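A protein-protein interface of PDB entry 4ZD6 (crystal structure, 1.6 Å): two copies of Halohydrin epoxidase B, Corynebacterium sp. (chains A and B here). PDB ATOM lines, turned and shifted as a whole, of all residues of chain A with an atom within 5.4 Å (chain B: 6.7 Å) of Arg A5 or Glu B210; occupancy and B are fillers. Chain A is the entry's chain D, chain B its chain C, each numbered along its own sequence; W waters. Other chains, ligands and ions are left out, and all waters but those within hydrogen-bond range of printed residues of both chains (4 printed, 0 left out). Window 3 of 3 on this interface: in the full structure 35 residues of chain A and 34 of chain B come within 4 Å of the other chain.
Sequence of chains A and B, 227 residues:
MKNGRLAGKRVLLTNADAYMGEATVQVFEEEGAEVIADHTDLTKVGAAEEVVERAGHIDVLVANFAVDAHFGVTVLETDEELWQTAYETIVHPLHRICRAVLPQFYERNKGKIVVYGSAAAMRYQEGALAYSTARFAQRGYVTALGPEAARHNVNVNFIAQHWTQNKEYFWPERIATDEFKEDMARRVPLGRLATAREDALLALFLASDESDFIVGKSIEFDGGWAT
The guanidinium group (NH1) of Arg B5 lies within salt-bridge range of the side-chain carboxylate (OE1) of Glu A210 (3.4 Å).
The guanidinium group (NH1) of Arg A5 is in salt-bridge range of the side-chain carboxylate (OE1) of Glu B210, at 3.3 Å.
The guanidinium group (NH2) of Arg A5 sits close to the guanidinium group (NH2) of Arg B5 (3.3 Å).
OD1 of Asp B212 lies within salt-bridge range of NZ of Lys B112, at 2.6 Å.
The side-chain hydroxyl of Ser B208 sits at hydrogen-bond distance from the backbone carbonyl oxygen of Phe B205.
OG of Ser B211 lies within hydrogen-bond range of O of Phe B205 (2.8 Å).
The backbone NH of Arg A5 sits at hydrogen-bond distance from the side-chain carboxylate of Glu A31 (2.9 Å).
NE of Arg A5 is in salt-bridge range of OE2 of Glu A210, 2.8 Å away.
N of Glu A210 lies close to OG of Ser A208 (3.2 Å).
Among the printed residues, pairs that only touch across the chains: Leu A202 with Phe B205 (3.7 Å), Glu A198 with Asp B212 (3.8 Å) and Leu A201 with Phe B205 (3.95 Å).
Of the printed residues of chain B, Leu A202 touches Phe B205.
Asp A209 touches none of the printed residues of chain B.
Printed residues of chain A within 4 Å of Phe B205: Leu A201 (3.95 Å) and Leu A202 (3.7 Å).
Of the printed residues of chain A, Glu B210 touches Arg A5.
Phe B213 touches none of the printed residues of chain A.
The nearest printed residue of chain A that does not touch Glu B210 is Leu A201 (4.001 Å).
The nearest printed residue of chain A that does not touch Arg B5 is Phe A205 (5.3 Å).
Hydrophobic or aromatic side chains of chain B within 4 Å of the printed part of chain A: Phe B205.
Hydrophobic or aromatic side chains of chain A within 4 Å of the printed part of chain B: Leu A202.
Among the printed residues, 6 pairs touch across the chains.
Among the printed residues, Asp or Glu carboxylates within 4 Å of a Lys or Arg side-chain nitrogen of the other chain: Arg A5 with Glu B210 and Glu A210 with Arg B5.
Arg B5 touches its own counterpart, Arg A5.
Arg A5 touches Glu B210, and with the chains exchanged Glu A210 touches Arg B5.
Water W1 lies within hydrogen-bond range of O of Glu B210 (2.7 Å) and O of Glu A198 (2.9 Å).
Water W4 lies within hydrogen-bond range of OE1 of Glu B210 (2.7 Å), O of Leu A201 (2.8 Å) and NH2 of Arg A5 (2.9 Å).
Water W2 lies within hydrogen-bond range of OE2 of Glu A198, N of Asp B212 and O of Asp B209.
Water W3 bridges the side-chain carboxylate of Glu A210 (2.8 Å) and the guanidinium group of Arg B5 (3.0 Å).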
ATOM      1  N   GLY A   4       6.933  30.276  13.644  1.00  0.00           N
ATOM      2  CA  GLY A   4       6.396  30.468  14.979  1.00  0.00           C
ATOM      3  C   GLY A   4       5.044  29.814  15.198  1.00  0.00           C
ATOM      4  O   GLY A   4       4.342  29.472  14.248  1.00  0.00           O
ATOM      5  N   ARG A   5       4.664  29.661  16.465  1.00  0.00           N
ATOM      6  CA  ARG A   5       3.429  28.956  16.782  1.00  0.00           C
ATOM      7  C   ARG A   5       2.178  29.780  16.506  1.00  0.00           C
ATOM      8  O   ARG A   5       1.081  29.215  16.473  1.00  0.00           O
ATOM      9  CB  ARG A   5       3.474  28.500  18.241  1.00  0.00           C
ATOM     10  CG  ARG A   5       4.489  27.377  18.433  1.00  0.00           C
ATOM     11  CD  ARG A   5       4.838  27.139  19.877  1.00  0.00           C
ATOM     12  NE  ARG A   5       3.670  26.699  20.626  1.00  0.00           N
ATOM     13  CZ  ARG A   5       3.623  26.664  21.949  1.00  0.00           C
ATOM     14  NH1 ARG A   5       4.680  27.050  22.649  1.00  0.00           N
ATOM     15  NH2 ARG A   5       2.518  26.254  22.567  1.00  0.00           N
ATOM     16  N   LEU A   6       2.320  31.090  16.299  1.00  0.00           N
ATOM     17  CA  LEU A   6       1.220  31.965  15.911  1.00  0.00           C
ATOM     18  C   LEU A   6       1.526  32.642  14.578  1.00  0.00           C
ATOM     19  O   LEU A   6       1.149  33.791  14.361  1.00  0.00           O
ATOM     20  CB  LEU A   6       0.944  33.021  16.983  1.00  0.00           C
ATOM     21  CG  LEU A   6       0.533  32.527  18.373  1.00  0.00           C
ATOM     22  CD1 LEU A   6       0.386  33.696  19.339  1.00  0.00           C
ATOM     23  CD2 LEU A   6      -0.757  31.696  18.288  1.00  0.00           C
ATOM     24  N   ALA A   7       2.207  31.931  13.682  1.00  0.00           N
ATOM     25  CA  ALA A   7       2.649  32.542  12.435  1.00  0.00           C
ATOM     26  C   ALA A   7       1.454  33.006  11.616  1.00  0.00           C
ATOM     27  O   ALA A   7       0.471  32.272  11.447  1.00  0.00           O
ATOM     28  CB  ALA A   7       3.497  31.556  11.634  1.00  0.00           C
ATOM     29  N   GLU A  31       6.446  34.407  18.705  1.00  0.00           N
ATOM     30  CA  GLU A  31       5.912  33.274  17.962  1.00  0.00           C
ATOM     31  C   GLU A  31       5.262  33.699  16.647  1.00  0.00           C
ATOM     32  O   GLU A  31       4.493  32.931  16.061  1.00  0.00           O
ATOM     33  CB  GLU A  31       4.924  32.493  18.835  1.00  0.00           C
ATOM     34  CG  GLU A  31       5.558  31.895  20.084  1.00  0.00           C
ATOM     35  CD  GLU A  31       6.553  30.789  19.790  1.00  0.00           C
ATOM     36  OE1 GLU A  31       6.496  30.185  18.695  1.00  0.00           O
ATOM     37  OE2 GLU A  31       7.403  30.516  20.665  1.00  0.00           O
ATOM     38  N   GLY A  32       5.569  34.901  16.167  1.00  0.00           N
ATOM     39  CA  GLY A  32       5.153  35.328  14.848  1.00  0.00           C
ATOM     40  C   GLY A  32       3.842  36.080  14.772  1.00  0.00           C
ATOM     41  O   GLY A  32       3.418  36.436  13.665  1.00  0.00           O
ATOM     42  N   GLU A 198       5.603  33.037  32.018  1.00  0.00           N
ATOM     43  CA  GLU A 198       5.005  31.714  32.176  1.00  0.00           C
ATOM     44  C   GLU A 198       3.500  31.766  31.965  1.00  0.00           C
ATOM     45  O   GLU A 198       2.917  30.868  31.345  1.00  0.00           O
ATOM     46  CB  GLU A 198       5.336  31.141  33.558  1.00  0.00           C
ATOM     47  CG  GLU A 198       6.765  30.628  33.672  1.00  0.00           C
ATOM     48  CD  GLU A 198       7.118  30.169  35.080  1.00  0.00           C
ATOM     49  OE1 GLU A 198       6.893  30.940  36.033  1.00  0.00           O
ATOM     50  OE2 GLU A 198       7.635  29.038  35.222  1.00  0.00           O
ATOM     51  N   LEU A 201       2.872  32.038  28.284  1.00  0.00           N
ATOM     52  CA  LEU A 201       3.089  30.770  27.593  1.00  0.00           C
ATOM     53  C   LEU A 201       1.867  29.859  27.682  1.00  0.00           C
ATOM     54  O   LEU A 201       1.606  29.084  26.751  1.00  0.00           O
ATOM     55  CB  LEU A 201       4.330  30.067  28.149  1.00  0.00           C
ATOM     56  CG  LEU A 201       5.658  30.715  27.737  1.00  0.00           C
ATOM     57  CD1 LEU A 201       6.794  30.181  28.600  1.00  0.00           C
ATOM     58  CD2 LEU A 201       5.952  30.458  26.257  1.00  0.00           C
ATOM     59  N   LEU A 202       1.114  29.932  28.778  1.00  0.00           N
ATOM     60  CA  LEU A 202      -0.163  29.231  28.833  1.00  0.00           C
ATOM     61  C   LEU A 202      -1.171  29.872  27.892  1.00  0.00           C
ATOM     62  O   LEU A 202      -1.881  29.172  27.159  1.00  0.00           O
ATOM     63  CB  LEU A 202      -0.703  29.221  30.268  1.00  0.00           C
ATOM     64  CG  LEU A 202      -2.119  28.669  30.453  1.00  0.00           C
ATOM     65  CD1 LEU A 202      -2.218  27.277  29.893  1.00  0.00           C
ATOM     66  CD2 LEU A 202      -2.493  28.678  31.930  1.00  0.00           C
ATOM     67  N   LEU A 204      -0.428  31.447  25.245  1.00  0.00           N
ATOM     68  CA  LEU A 204       0.037  31.077  23.909  1.00  0.00           C
ATOM     69  C   LEU A 204      -0.521  29.726  23.483  1.00  0.00           C
ATOM     70  O   LEU A 204      -1.027  29.574  22.366  1.00  0.00           O
ATOM     71  CB  LEU A 204       1.567  31.065  23.872  1.00  0.00           C
ATOM     72  CG  LEU A 204       2.253  30.395  22.691  1.00  0.00           C
ATOM     73  CD1 LEU A 204       1.857  31.084  21.394  1.00  0.00           C
ATOM     74  CD2 LEU A 204       3.760  30.498  22.896  1.00  0.00           C
ATOM     75  N   PHE A 205      -0.439  28.726  24.366  1.00  0.00           N
ATOM     76  CA  PHE A 205      -1.002  27.423  24.039  1.00  0.00           C
ATOM     77  C   PHE A 205      -2.485  27.547  23.717  1.00  0.00           C
ATOM     78  O   PHE A 205      -2.955  27.044  22.691  1.00  0.00           O
ATOM     79  CB  PHE A 205      -0.768  26.452  25.198  1.00  0.00           C
ATOM     80  CG  PHE A 205      -1.489  25.144  25.050  1.00  0.00           C
ATOM     81  CD1 PHE A 205      -1.077  24.213  24.114  1.00  0.00           C
ATOM     82  CD2 PHE A 205      -2.581  24.845  25.850  1.00  0.00           C
ATOM     83  CE1 PHE A 205      -1.740  22.995  23.980  1.00  0.00           C
ATOM     84  CE2 PHE A 205      -3.243  23.640  25.714  1.00  0.00           C
ATOM     85  CZ  PHE A 205      -2.820  22.716  24.771  1.00  0.00           C
ATOM     86  N   SER A 208      -3.211  29.222  20.352  1.00  0.00           N
ATOM     87  CA  SER A 208      -2.649  28.548  19.194  1.00  0.00           C
ATOM     88  C   SER A 208      -3.601  27.476  18.685  1.00  0.00           C
ATOM     89  O   SER A 208      -4.532  27.054  19.371  1.00  0.00           O
ATOM     90  CB  SER A 208      -1.305  27.919  19.549  1.00  0.00           C
ATOM     91  OG  SER A 208      -1.511  26.695  20.238  1.00  0.00           O
ATOM     92  N   ASP A 209      -3.337  27.006  17.472  1.00  0.00           N
ATOM     93  CA  ASP A 209      -4.145  25.937  16.898  1.00  0.00           C
ATOM     94  C   ASP A 209      -3.759  24.561  17.420  1.00  0.00           C
ATOM     95  O   ASP A 209      -4.244  23.547  16.905  1.00  0.00           O
ATOM     96  CB  ASP A 209      -4.062  25.983  15.369  1.00  0.00           C
ATOM     97  CG  ASP A 209      -4.800  27.167  14.794  1.00  0.00           C
ATOM     98  OD1 ASP A 209      -5.702  27.708  15.472  1.00  0.00           O
ATOM     99  OD2 ASP A 209      -4.478  27.565  13.655  1.00  0.00           O
ATOM    100  N   GLU A 210      -2.922  24.509  18.448  1.00  0.00           N
ATOM    101  CA  GLU A 210      -2.615  23.275  19.150  1.00  0.00           C
ATOM    102  C   GLU A 210      -3.649  22.937  20.209  1.00  0.00           C
ATOM    103  O   GLU A 210      -3.540  21.869  20.815  1.00  0.00           O
ATOM    104  CB  GLU A 210      -1.244  23.372  19.829  1.00  0.00           C
ATOM    105  CG  GLU A 210      -0.126  23.880  18.946  1.00  0.00           C
ATOM    106  CD  GLU A 210       1.001  24.543  19.738  1.00  0.00           C
ATOM    107  OE1 GLU A 210       1.057  24.366  20.975  1.00  0.00           O
ATOM    108  OE2 GLU A 210       1.824  25.260  19.122  1.00  0.00           O
ATOM    109  N   ARG B   5      10.787  21.997  21.366  1.00  0.00           N
ATOM    110  CA  ARG B   5      10.300  22.339  22.694  1.00  0.00           C
ATOM    111  C   ARG B   5      10.691  21.322  23.764  1.00  0.00           C
ATOM    112  O   ARG B   5      10.603  21.643  24.957  1.00  0.00           O
ATOM    113  CB  ARG B   5       8.788  22.519  22.614  1.00  0.00           C
ATOM    114  CG  ARG B   5       8.435  23.717  21.745  1.00  0.00           C
ATOM    115  CD  ARG B   5       6.966  23.721  21.374  1.00  0.00           C
ATOM    116  NE  ARG B   5       6.128  23.728  22.567  1.00  0.00           N
ATOM    117  CZ  ARG B   5       4.818  23.514  22.545  1.00  0.00           C
ATOM    118  NH1 ARG B   5       4.210  23.258  21.389  1.00  0.00           N
ATOM    119  NH2 ARG B   5       4.121  23.543  23.676  1.00  0.00           N
ATOM    120  N   LEU B   6      11.136  20.125  23.374  1.00  0.00           N
ATOM    121  CA  LEU B   6      11.682  19.141  24.300  1.00  0.00           C
ATOM    122  C   LEU B   6      13.127  18.799  23.945  1.00  0.00           C
ATOM    123  O   LEU B   6      13.569  17.667  24.135  1.00  0.00           O
ATOM    124  CB  LEU B   6      10.828  17.875  24.321  1.00  0.00           C
ATOM    125  CG  LEU B   6       9.381  18.044  24.785  1.00  0.00           C
ATOM    126  CD1 LEU B   6       8.605  16.743  24.655  1.00  0.00           C
ATOM    127  CD2 LEU B   6       9.354  18.537  26.223  1.00  0.00           C
ATOM    128  N   LYS B 112       8.866  16.004  35.515  1.00  0.00           N
ATOM    129  CA  LYS B 112       7.604  16.169  34.801  1.00  0.00           C
ATOM    130  C   LYS B 112       6.899  14.823  34.730  1.00  0.00           C
ATOM    131  O   LYS B 112       7.507  13.830  34.331  1.00  0.00           O
ATOM    132  CB  LYS B 112       7.842  16.711  33.383  1.00  0.00           C
ATOM    133  CG  LYS B 112       8.396  18.118  33.332  1.00  0.00           C
ATOM    134  CD  LYS B 112       7.305  19.154  33.527  1.00  0.00           C
ATOM    135  CE  LYS B 112       7.878  20.537  33.439  1.00  0.00           C
ATOM    136  NZ  LYS B 112       6.817  21.582  33.520  1.00  0.00           N
ATOM    137  N   LEU B 204       2.419  17.481  25.392  1.00  0.00           N
ATOM    138  CA  LEU B 204       3.660  18.185  25.097  1.00  0.00           C
ATOM    139  C   LEU B 204       3.788  19.457  25.932  1.00  0.00           C
ATOM    140  O   LEU B 204       4.818  19.684  26.574  1.00  0.00           O
ATOM    141  CB  LEU B 204       3.730  18.491  23.597  1.00  0.00           C
ATOM    142  CG  LEU B 204       4.793  19.489  23.137  1.00  0.00           C
ATOM    143  CD1 LEU B 204       6.212  18.963  23.330  1.00  0.00           C
ATOM    144  CD2 LEU B 204       4.549  19.821  21.682  1.00  0.00           C
ATOM    145  N   PHE B 205       2.742  20.290  25.955  1.00  0.00           N
ATOM    146  CA  PHE B 205       2.772  21.495  26.776  1.00  0.00           C
ATOM    147  C   PHE B 205       3.055  21.152  28.238  1.00  0.00           C
ATOM    148  O   PHE B 205       3.932  21.756  28.868  1.00  0.00           O
ATOM    149  CB  PHE B 205       1.447  22.252  26.632  1.00  0.00           C
ATOM    150  CG  PHE B 205       1.277  23.351  27.628  1.00  0.00           C
ATOM    151  CD1 PHE B 205       2.041  24.503  27.541  1.00  0.00           C
ATOM    152  CD2 PHE B 205       0.377  23.223  28.679  1.00  0.00           C
ATOM    153  CE1 PHE B 205       1.898  25.530  28.459  1.00  0.00           C
ATOM    154  CE2 PHE B 205       0.246  24.240  29.617  1.00  0.00           C
ATOM    155  CZ  PHE B 205       1.002  25.395  29.509  1.00  0.00           C
ATOM    156  N   ALA B 207       4.493  18.565  29.464  1.00  0.00           N
ATOM    157  CA  ALA B 207       5.796  17.938  29.642  1.00  0.00           C
ATOM    158  C   ALA B 207       6.939  18.917  29.444  1.00  0.00           C
ATOM    159  O   ALA B 207       8.063  18.643  29.882  1.00  0.00           O
ATOM    160  CB  ALA B 207       5.951  16.767  28.662  1.00  0.00           C
ATOM    161  N   SER B 208       6.663  20.052  28.817  1.00  0.00           N
ATOM    162  CA  SER B 208       7.683  21.033  28.500  1.00  0.00           C
ATOM    163  C   SER B 208       7.950  21.938  29.699  1.00  0.00           C
ATOM    164  O   SER B 208       7.185  21.987  30.664  1.00  0.00           O
ATOM    165  CB  SER B 208       7.245  21.864  27.297  1.00  0.00           C
ATOM    166  OG  SER B 208       6.305  22.849  27.692  1.00  0.00           O
ATOM    167  N   ASP B 209       9.042  22.687  29.619  1.00  0.00           N
ATOM    168  CA  ASP B 209       9.346  23.665  30.659  1.00  0.00           C
ATOM    169  C   ASP B 209       8.547  24.960  30.502  1.00  0.00           C
ATOM    170  O   ASP B 209       8.827  25.933  31.204  1.00  0.00           O
ATOM    171  CB  ASP B 209      10.852  23.953  30.684  1.00  0.00           C
ATOM    172  CG  ASP B 209      11.674  22.778  31.219  1.00  0.00           C
ATOM    173  OD1 ASP B 209      11.149  21.960  32.011  1.00  0.00           O
ATOM    174  OD2 ASP B 209      12.868  22.673  30.851  1.00  0.00           O
ATOM    175  N   GLU B 210       7.554  24.983  29.605  1.00  0.00           N
ATOM    176  CA  GLU B 210       6.617  26.093  29.506  1.00  0.00           C
ATOM    177  C   GLU B 210       5.481  25.997  30.515  1.00  0.00           C
ATOM    178  O   GLU B 210       4.682  26.930  30.608  1.00  0.00           O
ATOM    179  CB  GLU B 210       6.022  26.150  28.101  1.00  0.00           C
ATOM    180  CG  GLU B 210       7.067  26.102  26.996  1.00  0.00           C
ATOM    181  CD  GLU B 210       6.494  25.583  25.696  1.00  0.00           C
ATOM    182  OE1 GLU B 210       5.248  25.527  25.573  1.00  0.00           O
ATOM    183  OE2 GLU B 210       7.288  25.218  24.801  1.00  0.00           O
ATOM    184  N   SER B 211       5.401  24.899  31.279  1.00  0.00           N
ATOM    185  CA  SER B 211       4.237  24.613  32.115  1.00  0.00           C
ATOM    186  C   SER B 211       4.621  24.358  33.572  1.00  0.00           C
ATOM    187  O   SER B 211       3.872  23.692  34.301  1.00  0.00           O
ATOM    188  CB  SER B 211       3.465  23.413  31.563  1.00  0.00           C
ATOM    189  OG  SER B 211       4.272  22.240  31.580  1.00  0.00           O
ATOM    190  N   ASP B 212       5.764  24.882  34.014  1.00  0.00           N
ATOM    191  CA  ASP B 212       6.246  24.590  35.367  1.00  0.00           C
ATOM    192  C   ASP B 212       5.316  25.094  36.469  1.00  0.00           C
ATOM    193  O   ASP B 212       5.390  24.596  37.594  1.00  0.00           O
ATOM    194  CB  ASP B 212       7.630  25.208  35.582  1.00  0.00           C
ATOM    195  CG  ASP B 212       8.728  24.489  34.830  1.00  0.00           C
ATOM    196  OD1 ASP B 212       8.439  23.570  34.035  1.00  0.00           O
ATOM    197  OD2 ASP B 212       9.906  24.876  35.016  1.00  0.00           O
ATOM    198  N   PHE B 213       4.473  26.082  36.201  1.00  0.00           N
ATOM    199  CA  PHE B 213       3.604  26.579  37.257  1.00  0.00           C
ATOM    200  C   PHE B 213       2.327  25.763  37.414  1.00  0.00           C
ATOM    201  O   PHE B 213       1.517  26.086  38.290  1.00  0.00           O
ATOM    202  CB  PHE B 213       3.254  28.045  36.999  1.00  0.00           C
ATOM    203  CG  PHE B 213       2.971  28.837  38.238  1.00  0.00           C
ATOM    204  CD1 PHE B 213       3.914  28.932  39.262  1.00  0.00           C
ATOM    205  CD2 PHE B 213       1.786  29.537  38.360  1.00  0.00           C
ATOM    206  CE1 PHE B 213       3.647  29.705  40.399  1.00  0.00           C
ATOM    207  CE2 PHE B 213       1.525  30.306  39.478  1.00  0.00           C
ATOM    208  CZ  PHE B 213       2.445  30.386  40.496  1.00  0.00           C
ATOM    209  N   ILE B 214       2.118  24.726  36.610  1.00  0.00           N
ATOM    210  CA  ILE B 214       0.872  23.959  36.637  1.00  0.00           C
ATOM    211  C   ILE B 214       1.107  22.718  37.487  1.00  0.00           C
ATOM    212  O   ILE B 214       1.986  21.900  37.185  1.00  0.00           O
ATOM    213  CB  ILE B 214       0.396  23.620  35.218  1.00  0.00           C
ATOM    214  CG1 ILE B 214       0.200  24.919  34.415  1.00  0.00           C
ATOM    215  CG2 ILE B 214      -0.900  22.822  35.261  1.00  0.00           C
ATOM    216  CD1 ILE B 214      -0.152  24.701  32.970  1.00  0.00           C
HETATM  217  O   HOH W   1       2.493  28.056  31.685  1.00  0.00           O
HETATM  218  O   HOH W   2       7.085  27.354  33.147  1.00  0.00           O
HETATM  219  O   HOH W   3       1.601  22.271  22.763  1.00  0.00           O
HETATM  220  O   HOH W   4       3.101  27.157  25.314  1.00  0.00           O
